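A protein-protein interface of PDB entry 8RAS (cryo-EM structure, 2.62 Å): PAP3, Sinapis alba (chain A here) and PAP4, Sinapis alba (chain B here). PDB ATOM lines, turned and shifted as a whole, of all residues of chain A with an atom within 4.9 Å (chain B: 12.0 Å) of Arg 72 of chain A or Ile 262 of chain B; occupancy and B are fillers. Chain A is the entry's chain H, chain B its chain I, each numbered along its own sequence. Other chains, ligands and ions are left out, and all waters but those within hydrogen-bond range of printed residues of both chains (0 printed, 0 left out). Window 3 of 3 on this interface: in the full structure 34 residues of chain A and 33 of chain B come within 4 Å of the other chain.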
ATOM      1  N   GLU A  68      32.220   3.449 -12.582  1.00  0.00           N
ATOM      2  CA  GLU A  68      32.385   4.722 -13.281  1.00  0.00           C
ATOM      3  C   GLU A  68      31.036   5.359 -13.605  1.00  0.00           C
ATOM      4  O   GLU A  68      30.768   5.800 -14.721  1.00  0.00           O
ATOM      5  CB  GLU A  68      33.211   4.503 -14.544  1.00  0.00           C
ATOM      6  CG  GLU A  68      33.781   5.766 -15.166  1.00  0.00           C
ATOM      7  CD  GLU A  68      35.036   6.238 -14.475  1.00  0.00           C
ATOM      8  OE1 GLU A  68      35.676   5.425 -13.777  1.00  0.00           O
ATOM      9  OE2 GLU A  68      35.383   7.425 -14.633  1.00  0.00           O
ATOM     10  N   ASP A  69      30.169   5.394 -12.613  1.00  0.00           N
ATOM     11  CA  ASP A  69      28.986   6.244 -12.580  1.00  0.00           C
ATOM     12  C   ASP A  69      28.842   6.952 -11.245  1.00  0.00           C
ATOM     13  O   ASP A  69      28.411   8.107 -11.207  1.00  0.00           O
ATOM     14  CB  ASP A  69      27.720   5.428 -12.884  1.00  0.00           C
ATOM     15  CG  ASP A  69      27.562   4.235 -11.967  1.00  0.00           C
ATOM     16  OD1 ASP A  69      28.525   3.910 -11.243  1.00  0.00           O
ATOM     17  OD2 ASP A  69      26.475   3.620 -11.969  1.00  0.00           O
ATOM     18  N   GLU A  70      29.195   6.283 -10.149  1.00  0.00           N
ATOM     19  CA  GLU A  70      29.197   6.889  -8.826  1.00  0.00           C
ATOM     20  C   GLU A  70      30.503   7.599  -8.519  1.00  0.00           C
ATOM     21  O   GLU A  70      30.508   8.554  -7.736  1.00  0.00           O
ATOM     22  CB  GLU A  70      28.930   5.825  -7.758  1.00  0.00           C
ATOM     23  CG  GLU A  70      29.764   4.561  -7.916  1.00  0.00           C
ATOM     24  CD  GLU A  70      31.103   4.648  -7.208  1.00  0.00           C
ATOM     25  OE1 GLU A  70      31.262   5.530  -6.339  1.00  0.00           O
ATOM     26  OE2 GLU A  70      31.998   3.835  -7.522  1.00  0.00           O
ATOM     27  N   ALA A  71      31.612   7.149  -9.110  1.00  0.00           N
ATOM     28  CA  ALA A  71      32.877   7.855  -8.938  1.00  0.00           C
ATOM     29  C   ALA A  71      32.817   9.242  -9.561  1.00  0.00           C
ATOM     30  O   ALA A  71      33.310  10.211  -8.975  1.00  0.00           O
ATOM     31  CB  ALA A  71      34.019   7.042  -9.543  1.00  0.00           C
ATOM     32  N   ARG A  72      32.214   9.358 -10.745  1.00  0.00           N
ATOM     33  CA  ARG A  72      32.065  10.663 -11.382  1.00  0.00           C
ATOM     34  C   ARG A  72      31.158  11.576 -10.567  1.00  0.00           C
ATOM     35  O   ARG A  72      31.444  12.769 -10.406  1.00  0.00           O
ATOM     36  CB  ARG A  72      31.528  10.483 -12.800  1.00  0.00           C
ATOM     37  CG  ARG A  72      30.619  11.595 -13.278  1.00  0.00           C
ATOM     38  CD  ARG A  72      30.538  11.610 -14.792  1.00  0.00           C
ATOM     39  NE  ARG A  72      30.396  10.268 -15.342  1.00  0.00           N
ATOM     40  CZ  ARG A  72      29.257   9.589 -15.376  1.00  0.00           C
ATOM     41  NH1 ARG A  72      28.136  10.096 -14.893  1.00  0.00           N
ATOM     42  NH2 ARG A  72      29.244   8.370 -15.907  1.00  0.00           N
ATOM     43  N   ARG A  73      30.055  11.032 -10.047  1.00  0.00           N
ATOM     44  CA  ARG A  73      29.160  11.826  -9.211  1.00  0.00           C
ATOM     45  C   ARG A  73      29.860  12.285  -7.940  1.00  0.00           C
ATOM     46  O   ARG A  73      29.703  13.437  -7.513  1.00  0.00           O
ATOM     47  CB  ARG A  73      27.908  11.015  -8.878  1.00  0.00           C
ATOM     48  CG  ARG A  73      27.101  11.555  -7.713  1.00  0.00           C
ATOM     49  CD  ARG A  73      25.712  10.941  -7.675  1.00  0.00           C
ATOM     50  NE  ARG A  73      24.793  11.720  -6.856  1.00  0.00           N
ATOM     51  CZ  ARG A  73      23.963  12.639  -7.331  1.00  0.00           C
ATOM     52  NH1 ARG A  73      23.905  12.917  -8.622  1.00  0.00           N
ATOM     53  NH2 ARG A  73      23.171  13.294  -6.487  1.00  0.00           N
ATOM     54  N   ARG A  74      30.644  11.399  -7.325  1.00  0.00           N
ATOM     55  CA  ARG A  74      31.412  11.774  -6.144  1.00  0.00           C
ATOM     56  C   ARG A  74      32.435  12.851  -6.474  1.00  0.00           C
ATOM     57  O   ARG A  74      32.640  13.780  -5.687  1.00  0.00           O
ATOM     58  CB  ARG A  74      32.098  10.544  -5.554  1.00  0.00           C
ATOM     59  CG  ARG A  74      32.949  10.826  -4.329  1.00  0.00           C
ATOM     60  CD  ARG A  74      32.771   9.787  -3.221  1.00  0.00           C
ATOM     61  NE  ARG A  74      33.222   8.451  -3.598  1.00  0.00           N
ATOM     62  CZ  ARG A  74      32.463   7.527  -4.174  1.00  0.00           C
ATOM     63  NH1 ARG A  74      31.179   7.735  -4.411  1.00  0.00           N
ATOM     64  NH2 ARG A  74      33.004   6.358  -4.505  1.00  0.00           N
ATOM     65  N   ASN A  75      33.094  12.739  -7.628  1.00  0.00           N
ATOM     66  CA  ASN A  75      34.042  13.767  -8.042  1.00  0.00           C
ATOM     67  C   ASN A  75      33.348  15.113  -8.187  1.00  0.00           C
ATOM     68  O   ASN A  75      33.826  16.128  -7.671  1.00  0.00           O
ATOM     69  CB  ASN A  75      34.713  13.364  -9.355  1.00  0.00           C
ATOM     70  CG  ASN A  75      36.040  12.672  -9.143  1.00  0.00           C
ATOM     71  OD1 ASN A  75      36.559  12.628  -8.029  1.00  0.00           O
ATOM     72  ND2 ASN A  75      36.598  12.123 -10.214  1.00  0.00           N
ATOM     73  N   TRP A  76      32.197  15.130  -8.860  1.00  0.00           N
ATOM     74  CA  TRP A  76      31.447  16.371  -9.021  1.00  0.00           C
ATOM     75  C   TRP A  76      31.070  16.965  -7.669  1.00  0.00           C
ATOM     76  O   TRP A  76      31.272  18.159  -7.424  1.00  0.00           O
ATOM     77  CB  TRP A  76      30.199  16.120  -9.870  1.00  0.00           C
ATOM     78  CG  TRP A  76      29.257  17.295  -9.977  1.00  0.00           C
ATOM     79  CD1 TRP A  76      28.439  17.787  -8.999  1.00  0.00           C
ATOM     80  CD2 TRP A  76      29.029  18.111 -11.133  1.00  0.00           C
ATOM     81  NE1 TRP A  76      27.727  18.859  -9.470  1.00  0.00           N
ATOM     82  CE2 TRP A  76      28.068  19.077 -10.778  1.00  0.00           C
ATOM     83  CE3 TRP A  76      29.545  18.119 -12.431  1.00  0.00           C
ATOM     84  CZ2 TRP A  76      27.615  20.041 -11.673  1.00  0.00           C
ATOM     85  CZ3 TRP A  76      29.095  19.077 -13.315  1.00  0.00           C
ATOM     86  CH2 TRP A  76      28.139  20.023 -12.934  1.00  0.00           C
ATOM     87  N   TRP A  81      34.505  18.719  -9.693  1.00  0.00           N
ATOM     88  CA  TRP A  81      34.774  18.361 -11.079  1.00  0.00           C
ATOM     89  C   TRP A  81      33.638  18.818 -11.986  1.00  0.00           C
ATOM     90  O   TRP A  81      32.468  18.807 -11.596  1.00  0.00           O
ATOM     91  CB  TRP A  81      34.974  16.852 -11.213  1.00  0.00           C
ATOM     92  CG  TRP A  81      35.015  16.390 -12.635  1.00  0.00           C
ATOM     93  CD1 TRP A  81      36.106  16.347 -13.452  1.00  0.00           C
ATOM     94  CD2 TRP A  81      33.913  15.916 -13.417  1.00  0.00           C
ATOM     95  NE1 TRP A  81      35.753  15.874 -14.689  1.00  0.00           N
ATOM     96  CE2 TRP A  81      34.412  15.604 -14.694  1.00  0.00           C
ATOM     97  CE3 TRP A  81      32.552  15.728 -13.159  1.00  0.00           C
ATOM     98  CZ2 TRP A  81      33.600  15.110 -15.710  1.00  0.00           C
ATOM     99  CZ3 TRP A  81      31.749  15.239 -14.168  1.00  0.00           C
ATOM    100  CH2 TRP A  81      32.274  14.935 -15.428  1.00  0.00           C
ATOM    101  N   GLU B 257      19.029  17.678  -5.830  1.00  0.00           N
ATOM    102  CA  GLU B 257      20.206  16.963  -6.291  1.00  0.00           C
ATOM    103  C   GLU B 257      20.724  17.590  -7.576  1.00  0.00           C
ATOM    104  O   GLU B 257      19.939  18.088  -8.389  1.00  0.00           O
ATOM    105  CB  GLU B 257      19.896  15.478  -6.531  1.00  0.00           C
ATOM    106  CG  GLU B 257      19.578  14.701  -5.267  1.00  0.00           C
ATOM    107  CD  GLU B 257      20.778  14.564  -4.353  1.00  0.00           C
ATOM    108  OE1 GLU B 257      21.905  14.422  -4.870  1.00  0.00           O
ATOM    109  OE2 GLU B 257      20.594  14.598  -3.119  1.00  0.00           O
ATOM    110  N   PRO B 258      22.037  17.580  -7.787  1.00  0.00           N
ATOM    111  CA  PRO B 258      22.599  18.216  -8.981  1.00  0.00           C
ATOM    112  C   PRO B 258      22.491  17.339 -10.218  1.00  0.00           C
ATOM    113  O   PRO B 258      22.475  16.108 -10.145  1.00  0.00           O
ATOM    114  CB  PRO B 258      24.066  18.443  -8.598  1.00  0.00           C
ATOM    115  CG  PRO B 258      24.360  17.374  -7.611  1.00  0.00           C
ATOM    116  CD  PRO B 258      23.082  17.099  -6.866  1.00  0.00           C
ATOM    117  N   THR B 259      22.418  18.004 -11.369  1.00  0.00           N
ATOM    118  CA  THR B 259      22.423  17.335 -12.666  1.00  0.00           C
ATOM    119  C   THR B 259      23.872  17.193 -13.119  1.00  0.00           C
ATOM    120  O   THR B 259      24.543  18.191 -13.399  1.00  0.00           O
ATOM    121  CB  THR B 259      21.599  18.119 -13.685  1.00  0.00           C
ATOM    122  OG1 THR B 259      20.214  18.069 -13.322  1.00  0.00           O
ATOM    123  CG2 THR B 259      21.773  17.533 -15.076  1.00  0.00           C
ATOM    124  N   ILE B 260      24.350  15.960 -13.194  1.00  0.00           N
ATOM    125  CA  ILE B 260      25.757  15.659 -13.440  1.00  0.00           C
ATOM    126  C   ILE B 260      25.884  15.083 -14.845  1.00  0.00           C
ATOM    127  O   ILE B 260      25.230  14.080 -15.159  1.00  0.00           O
ATOM    128  CB  ILE B 260      26.314  14.688 -12.389  1.00  0.00           C
ATOM    129  CG1 ILE B 260      26.289  15.349 -11.011  1.00  0.00           C
ATOM    130  CG2 ILE B 260      27.719  14.256 -12.755  1.00  0.00           C
ATOM    131  CD1 ILE B 260      26.829  14.487  -9.908  1.00  0.00           C
ATOM    132  N   PRO B 261      26.698  15.676 -15.717  1.00  0.00           N
ATOM    133  CA  PRO B 261      26.835  15.151 -17.079  1.00  0.00           C
ATOM    134  C   PRO B 261      27.544  13.807 -17.100  1.00  0.00           C
ATOM    135  O   PRO B 261      28.312  13.457 -16.202  1.00  0.00           O
ATOM    136  CB  PRO B 261      27.665  16.224 -17.798  1.00  0.00           C
ATOM    137  CG  PRO B 261      27.764  17.381 -16.843  1.00  0.00           C
ATOM    138  CD  PRO B 261      27.580  16.825 -15.477  1.00  0.00           C
ATOM    139  N   ILE B 262      27.268  13.045 -18.162  1.00  0.00           N
ATOM    140  CA  ILE B 262      27.876  11.725 -18.329  1.00  0.00           C
ATOM    141  C   ILE B 262      29.301  11.779 -18.858  1.00  0.00           C
ATOM    142  O   ILE B 262      29.970  10.740 -18.908  1.00  0.00           O
ATOM    143  CB  ILE B 262      26.967  10.844 -19.210  1.00  0.00           C
ATOM    144  CG1 ILE B 262      26.479  11.558 -20.489  1.00  0.00           C
ATOM    145  CG2 ILE B 262      25.773  10.345 -18.409  1.00  0.00           C
ATOM    146  CD1 ILE B 262      27.530  12.138 -21.423  1.00  0.00           C
ATOM    147  N   ALA B 263      29.784  12.951 -19.258  1.00  0.00           N
ATOM    148  CA  ALA B 263      31.131  13.075 -19.801  1.00  0.00           C
ATOM    149  C   ALA B 263      32.172  13.017 -18.690  1.00  0.00           C
ATOM    150  O   ALA B 263      32.971  13.938 -18.527  1.00  0.00           O
ATOM    151  CB  ALA B 263      31.270  14.367 -20.592  1.00  0.00           C
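Of the 10 printed residues of chain A, 4 touch a printed residue of chain B.
Hydrophobic or aromatic side chains of chain A within 4 Å of the printed part of chain B: Trp 76 and Trp 81.
Among the printed residues, Asp or Glu carboxylates within 4 Å of a Lys or Arg side-chain nitrogen of the other chain: Arg 73 of chain A with Glu 257 of chain B (2.3 Å).
Ile 260 of chain B touches Arg 72 of chain A (CG2 to CG, 3.97 Å).
O of Pro 261 of chain B touches CD of Arg 72 of chain A, 3.2 Å away.
Ile 262 of chain B touches Arg 72 of chain A (O to NE, 3.6 Å).
Arg 73 of chain A touches Pro 258 of chain B (NH1 to O, 3.8 Å).
Ile 260 of chain B touches Arg 73 of chain A (CD1 to NH1, 3.6 Å).
Pro 258 of chain B touches Trp 76 of chain A.
Trp 76 of chain A touches Thr 259 of chain B.
CG of Trp 76 of chain A touches CG1 of Ile 260 of chain B, at 3.7 Å.
Pro 261 of chain B touches Trp 76 of chain A.
CZ2 of Trp 81 of chain A touches O of Ala 263 of chain B, at 3.1 Å.
Arg 72 of chain A touches just these residues of chain B: Ile 260 (3.97 Å), Pro 261 (3.2 Å) and Ile 262 (3.6 Å).
Of chain A, only Arg 72 (3.6 Å) comes within 4 Å of Ile 262 of chain B.
No residue of chain B comes within 4 Å of Glu 68 of chain A.
No residue of chain B comes within 4 Å of Asp 69 of chain A.
No residue of chain B comes within 4 Å of Glu 70 of chain A.
No residue of chain B comes within 4 Å of Ala 71 of chain A.
Asn 75 of chain A touches none of the printed residues of chain B.
Trp 81 of chain A touches one residue of chain B.
Printed residues of chain A within 4 Å of Thr 259 of chain B: Trp 76.
Of the printed residues of chain A, Ile 260 of chain B touches Arg 72, Arg 73 and Trp 76.
The nearest residue of chain B that does not touch Arg 72 of chain A is Ala 263 of chain B (4.5 Å).
The nearest printed residue of chain A that does not touch Ile 262 of chain B is Trp 81 of chain A (5.5 Å).
The backbone carbonyl oxygen (O) of Glu 68 of chain A sits at hydrogen-bond distance from the guanidinium group (NH2) of Arg 72 of chain A.
The backbone carbonyl oxygen of Asn 75 of chain A is in hydrogen-bond range of the backbone NH of Trp 81 of chain A.
The side-chain carboxylate of Glu 257 of chain B lies close to the guanidinium group of Arg 73 of chain A (2.3 Å).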
